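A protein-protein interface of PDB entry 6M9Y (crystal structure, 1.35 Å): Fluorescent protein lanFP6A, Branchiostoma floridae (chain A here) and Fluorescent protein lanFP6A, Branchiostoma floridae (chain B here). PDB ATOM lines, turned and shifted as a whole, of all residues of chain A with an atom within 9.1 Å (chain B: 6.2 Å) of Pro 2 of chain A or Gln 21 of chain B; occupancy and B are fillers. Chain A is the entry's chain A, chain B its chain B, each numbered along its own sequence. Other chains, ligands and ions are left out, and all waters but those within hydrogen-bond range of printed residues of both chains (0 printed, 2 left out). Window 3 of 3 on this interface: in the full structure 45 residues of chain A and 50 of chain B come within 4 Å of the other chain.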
ATOM      1  N   PRO A   2     -18.421   5.183  -5.763  1.00  0.00           N
ATOM      2  CA  PRO A   2     -18.530   3.756  -5.806  1.00  0.00           C
ATOM      3  C   PRO A   2     -17.229   3.079  -5.381  1.00  0.00           C
ATOM      4  O   PRO A   2     -16.221   3.758  -5.229  1.00  0.00           O
ATOM      5  CB  PRO A   2     -18.837   3.426  -7.273  1.00  0.00           C
ATOM      6  CG  PRO A   2     -18.698   4.709  -8.052  1.00  0.00           C
ATOM      7  CD  PRO A   2     -18.508   5.830  -7.068  1.00  0.00           C
ATOM      8  N   LEU A   3     -17.294   1.765  -5.164  1.00  0.00           N
ATOM      9  CA  LEU A   3     -16.099   0.939  -4.967  1.00  0.00           C
ATOM     10  C   LEU A   3     -15.434   0.813  -6.315  1.00  0.00           C
ATOM     11  O   LEU A   3     -16.089   0.887  -7.367  1.00  0.00           O
ATOM     12  CB  LEU A   3     -16.454  -0.453  -4.426  1.00  0.00           C
ATOM     13  CG  LEU A   3     -16.987  -0.523  -2.993  1.00  0.00           C
ATOM     14  CD1 LEU A   3     -17.360  -1.966  -2.685  1.00  0.00           C
ATOM     15  CD2 LEU A   3     -16.001  -0.010  -1.945  1.00  0.00           C
ATOM     16  N   PRO A   4     -14.133   0.509  -6.354  1.00  0.00           N
ATOM     17  CA  PRO A   4     -13.457   0.434  -7.642  1.00  0.00           C
ATOM     18  C   PRO A   4     -13.655  -0.897  -8.386  1.00  0.00           C
ATOM     19  O   PRO A   4     -13.846  -1.971  -7.761  1.00  0.00           O
ATOM     20  CB  PRO A   4     -11.984   0.550  -7.246  1.00  0.00           C
ATOM     21  CG  PRO A   4     -11.932  -0.113  -5.900  1.00  0.00           C
ATOM     22  CD  PRO A   4     -13.208   0.347  -5.211  1.00  0.00           C
ATOM     23  N   LYS A   5     -13.601  -0.785  -9.708  1.00  0.00           N
ATOM     24  CA  LYS A   5     -13.635  -1.930 -10.570  1.00  0.00           C
ATOM     25  C   LYS A   5     -12.428  -1.988 -11.501  1.00  0.00           C
ATOM     26  O   LYS A   5     -12.069  -3.083 -11.960  1.00  0.00           O
ATOM     27  CB  LYS A   5     -14.865  -1.958 -11.498  1.00  0.00           C
ATOM     28  CG  LYS A   5     -16.220  -1.936 -10.814  1.00  0.00           C
ATOM     29  CD  LYS A   5     -17.384  -1.961 -11.816  1.00  0.00           C
ATOM     30  CE  LYS A   5     -18.719  -1.664 -11.184  1.00  0.00           C
ATOM     31  NZ  LYS A   5     -19.765  -1.667 -12.232  1.00  0.00           N
ATOM     32  N   PRO A  30     -13.221  -5.507  -5.249  1.00  0.00           N
ATOM     33  CA  PRO A  30     -13.093  -4.786  -3.986  1.00  0.00           C
ATOM     34  C   PRO A  30     -13.826  -5.487  -2.841  1.00  0.00           C
ATOM     35  O   PRO A  30     -13.672  -5.091  -1.682  1.00  0.00           O
ATOM     36  CB  PRO A  30     -13.736  -3.427  -4.286  1.00  0.00           C
ATOM     37  CG  PRO A  30     -14.798  -3.724  -5.323  1.00  0.00           C
ATOM     38  CD  PRO A  30     -14.215  -4.872  -6.135  1.00  0.00           C
ATOM     39  N   ASN A  31     -14.542  -6.573  -3.164  1.00  0.00           N
ATOM     40  CA  ASN A  31     -15.156  -7.416  -2.130  1.00  0.00           C
ATOM     41  C   ASN A  31     -14.232  -8.585  -1.739  1.00  0.00           C
ATOM     42  O   ASN A  31     -14.533  -9.303  -0.771  1.00  0.00           O
ATOM     43  CB  ASN A  31     -16.556  -7.878  -2.559  1.00  0.00           C
ATOM     44  CG  ASN A  31     -17.475  -6.694  -2.848  1.00  0.00           C
ATOM     45  OD1 ASN A  31     -17.980  -6.533  -3.957  1.00  0.00           O
ATOM     46  ND2 ASN A  31     -17.705  -5.855  -1.854  1.00  0.00           N
ATOM     47  N   MET B  13     -16.139  -1.734   4.992  1.00  0.00           N
ATOM     48  CA  MET B  13     -15.190  -1.068   4.097  1.00  0.00           C
ATOM     49  C   MET B  13     -13.885  -0.824   4.846  1.00  0.00           C
ATOM     50  O   MET B  13     -13.881  -0.435   6.010  1.00  0.00           O
ATOM     51  CB  MET B  13     -15.668   0.323   3.676  1.00  0.00           C
ATOM     52  CG  MET B  13     -16.685   0.328   2.577  1.00  0.00           C
ATOM     53  SD  MET B  13     -17.026   2.029   1.991  1.00  0.00           S
ATOM     54  CE  MET B  13     -17.770   2.777   3.443  1.00  0.00           C
ATOM     55  N   PHE B  16      -9.491   2.884   3.153  1.00  0.00           N
ATOM     56  CA  PHE B  16      -9.128   3.249   1.805  1.00  0.00           C
ATOM     57  C   PHE B  16     -10.407   3.353   0.937  1.00  0.00           C
ATOM     58  O   PHE B  16     -10.601   4.304   0.179  1.00  0.00           O
ATOM     59  CB  PHE B  16      -8.142   2.237   1.203  1.00  0.00           C
ATOM     60  CG  PHE B  16      -7.014   1.876   2.119  1.00  0.00           C
ATOM     61  CD1 PHE B  16      -5.950   2.741   2.270  1.00  0.00           C
ATOM     62  CD2 PHE B  16      -7.026   0.673   2.811  1.00  0.00           C
ATOM     63  CE1 PHE B  16      -4.895   2.396   3.094  1.00  0.00           C
ATOM     64  CE2 PHE B  16      -5.976   0.334   3.657  1.00  0.00           C
ATOM     65  CZ  PHE B  16      -4.927   1.207   3.797  1.00  0.00           C
ATOM     66  N   GLN B  17     -11.281   2.361   1.115  1.00  0.00           N
ATOM     67  CA  GLN B  17     -12.567   2.293   0.408  1.00  0.00           C
ATOM     68  C   GLN B  17     -13.485   3.442   0.819  1.00  0.00           C
ATOM     69  O   GLN B  17     -14.138   4.066  -0.030  1.00  0.00           O
ATOM     70  CB  GLN B  17     -13.221   0.918   0.631  1.00  0.00           C
ATOM     71  CG  GLN B  17     -12.490  -0.175  -0.125  1.00  0.00           C
ATOM     72  CD  GLN B  17     -13.077  -1.545   0.054  1.00  0.00           C
ATOM     73  OE1 GLN B  17     -13.693  -1.864   1.091  1.00  0.00           O
ATOM     74  NE2 GLN B  17     -12.834  -2.381  -0.958  1.00  0.00           N
ATOM     75  N   ALA B  18     -13.539   3.732   2.119  1.00  0.00           N
ATOM     76  CA  ALA B  18     -14.430   4.770   2.613  1.00  0.00           C
ATOM     77  C   ALA B  18     -14.008   6.132   2.064  1.00  0.00           C
ATOM     78  O   ALA B  18     -14.848   6.939   1.728  1.00  0.00           O
ATOM     79  CB  ALA B  18     -14.396   4.783   4.104  1.00  0.00           C
ATOM     80  N   ALA B  19     -12.695   6.363   1.980  1.00  0.00           N
ATOM     81  CA  ALA B  19     -12.149   7.620   1.491  1.00  0.00           C
ATOM     82  C   ALA B  19     -12.347   7.783  -0.023  1.00  0.00           C
ATOM     83  O   ALA B  19     -12.368   8.908  -0.537  1.00  0.00           O
ATOM     84  CB  ALA B  19     -10.686   7.741   1.879  1.00  0.00           C
ATOM     85  N   MET B  20     -12.418   6.691  -0.773  1.00  0.00           N
ATOM     86  CA  MET B  20     -12.796   6.783  -2.180  1.00  0.00           C
ATOM     87  C   MET B  20     -14.308   7.069  -2.283  1.00  0.00           C
ATOM     88  O   MET B  20     -14.727   7.943  -3.055  1.00  0.00           O
ATOM     89  CB  MET B  20     -12.472   5.484  -2.902  1.00  0.00           C
ATOM     90  CG  MET B  20     -12.919   5.448  -4.359  1.00  0.00           C
ATOM     91  SD  MET B  20     -12.339   3.954  -5.165  1.00  0.00           S
ATOM     92  CE  MET B  20     -13.168   4.160  -6.752  1.00  0.00           C
ATOM     93  N   GLN B  21     -15.132   6.326  -1.535  1.00  0.00           N
ATOM     94  CA  GLN B  21     -16.569   6.424  -1.622  1.00  0.00           C
ATOM     95  C   GLN B  21     -17.021   7.844  -1.310  1.00  0.00           C
ATOM     96  O   GLN B  21     -17.926   8.354  -1.948  1.00  0.00           O
ATOM     97  CB  GLN B  21     -17.245   5.482  -0.630  1.00  0.00           C
ATOM     98  CG  GLN B  21     -17.221   4.030  -1.068  1.00  0.00           C
ATOM     99  CD  GLN B  21     -18.319   3.636  -2.017  1.00  0.00           C
ATOM    100  OE1 GLN B  21     -18.691   4.392  -2.926  1.00  0.00           O
ATOM    101  NE2 GLN B  21     -18.847   2.435  -1.805  1.00  0.00           N
ATOM    102  N   ASP B  22     -16.440   8.469  -0.279  1.00  0.00           N
ATOM    103  CA  ASP B  22     -16.914   9.832   0.124  1.00  0.00           C
ATOM    104  C   ASP B  22     -16.173  10.956  -0.593  1.00  0.00           C
ATOM    105  O   ASP B  22     -16.379  12.138  -0.287  1.00  0.00           O
ATOM    106  CB  ASP B  22     -16.958   9.972   1.639  1.00  0.00           C
ATOM    107  CG  ASP B  22     -15.607  10.116   2.304  1.00  0.00           C
ATOM    108  OD1 ASP B  22     -14.611  10.225   1.542  1.00  0.00           O
ATOM    109  OD2 ASP B  22     -15.569  10.179   3.564  1.00  0.00           O
ATOM    110  N   GLU B  23     -15.318  10.597  -1.542  1.00  0.00           N
ATOM    111  CA  GLU B  23     -14.589  11.539  -2.402  1.00  0.00           C
ATOM    112  C   GLU B  23     -13.595  12.420  -1.602  1.00  0.00           C
ATOM    113  O   GLU B  23     -13.201  13.476  -2.101  1.00  0.00           O
ATOM    114  CB  GLU B  23     -15.579  12.398  -3.202  1.00  0.00           C
ATOM    115  CG  GLU B  23     -16.538  11.564  -4.059  1.00  0.00           C
ATOM    116  CD  GLU B  23     -17.567  12.393  -4.840  1.00  0.00           C
ATOM    117  OE1 GLU B  23     -17.143  13.275  -5.615  1.00  0.00           O
ATOM    118  OE2 GLU B  23     -18.797  12.206  -4.667  1.00  0.00           O
ATOM    119  N   SER B  24     -13.107  11.972  -0.425  1.00  0.00           N
ATOM    120  CA  SER B  24     -12.135  12.761   0.384  1.00  0.00           C
ATOM    121  C   SER B  24     -10.674  12.334   0.113  1.00  0.00           C
ATOM    122  O   SER B  24      -9.810  13.164   0.064  1.00  0.00           O
ATOM    123  CB  SER B  24     -12.492  12.684   1.850  1.00  0.00           C
ATOM    124  OG  SER B  24     -12.471  11.338   2.336  1.00  0.00           O
ATOM    125  N   GLY B  50     -15.433   7.834 -10.826  1.00  0.00           N
ATOM    126  CA  GLY B  50     -16.365   6.840 -10.405  1.00  0.00           C
ATOM    127  C   GLY B  50     -15.674   5.582  -9.897  1.00  0.00           C
ATOM    128  O   GLY B  50     -14.853   5.662  -8.991  1.00  0.00           O
ATOM    129  N   SER B  51     -15.936   4.454 -10.555  1.00  0.00           N
ATOM    130  CA  SER B  51     -15.350   3.171 -10.155  1.00  0.00           C
ATOM    131  C   SER B  51     -13.950   2.959 -10.748  1.00  0.00           C
ATOM    132  O   SER B  51     -13.361   1.893 -10.573  1.00  0.00           O
ATOM    133  CB  SER B  51     -16.236   2.031 -10.594  1.00  0.00           C
ATOM    134  OG  SER B  51     -16.292   1.952 -12.026  1.00  0.00           O
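Pro 2 of chain A touches Met 20 of chain B. Pro 2 of chain A touches Gly 50 of chain B (CG to C, 3.6 Å). Ser 51 of chain B touches Pro 2 of chain A. CD of Gln 17 of chain B touches CD2 of Leu 3 of chain A (3.9 Å). Gln 21 of chain B touches Leu 3 of chain A (NE2 to CG, 3.7 Å). O of Leu 3 of chain A touches CB of Ser 51 of chain B (3.4 Å). Pro 4 of chain A touches Met 20 of chain B. Pro 4 of chain A touches Ser 51 of chain B.
Of the 6 printed residues of chain A, 5 touch a printed residue of chain B. Hydrophobic or aromatic side chains of chain A that line the printed part of chain B: Pro 2, Leu 3, Pro 4 and Pro 30. Hydrophobic or aromatic side chains of chain B that line the printed part of chain A: Met 20. Among the printed residues, 11 pairs touch across the chains. Among the printed residues, no Asp or Glu carboxylate lies within 4 Å of a Lys or Arg side-chain nitrogen of the other chain.
The backbone carbonyl oxygen (O) of Pro 2 of chain A sits close to the side-chain amide oxygen (OE1) of Gln 21 of chain B, at 3.4 Å. N of Lys 5 of chain A lies within hydrogen-bond range of O of Ser 51 of chain B (2.8 Å). NE2 of Gln 17 of chain B is in hydrogen-bond range of O of Pro 30 of chain A (2.9 Å).
Pro 2 of chain A touches four residues of chain B. Gln 21 of chain B touches two residues of chain A. Met 20 of chain B touches just these residues of chain A: Pro 2 (3.4 Å) and Pro 4 (3.7 Å). Printed residues of chain B within 4 Å of Leu 3 of chain A: Gln 17 (3.9 Å), Gln 21 (3.7 Å) and Ser 51 (3.4 Å). Of the printed residues of chain A, Ser 51 of chain B touches Pro 2, Leu 3, Pro 4 and Lys 5. Printed residues of chain A within 4 Å of Gln 17 of chain B: Leu 3 and Pro 30. Of the printed residues of chain A, Gly 50 of chain B touches Pro 2. Printed residues of chain B within 4 Å of Pro 4 of chain A: Met 20 and Ser 51. Asp 22 of chain B touches none of the printed residues of chain A. Ala 18 of chain B touches none of the printed residues of chain A. The nearest residue of chain A that does not touch Gln 21 of chain B is Pro 4 of chain A (6.8 Å). The nearest printed residue of chain A that does not touch Ser 51 of chain B is Pro 30 of chain A (7.8 Å).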
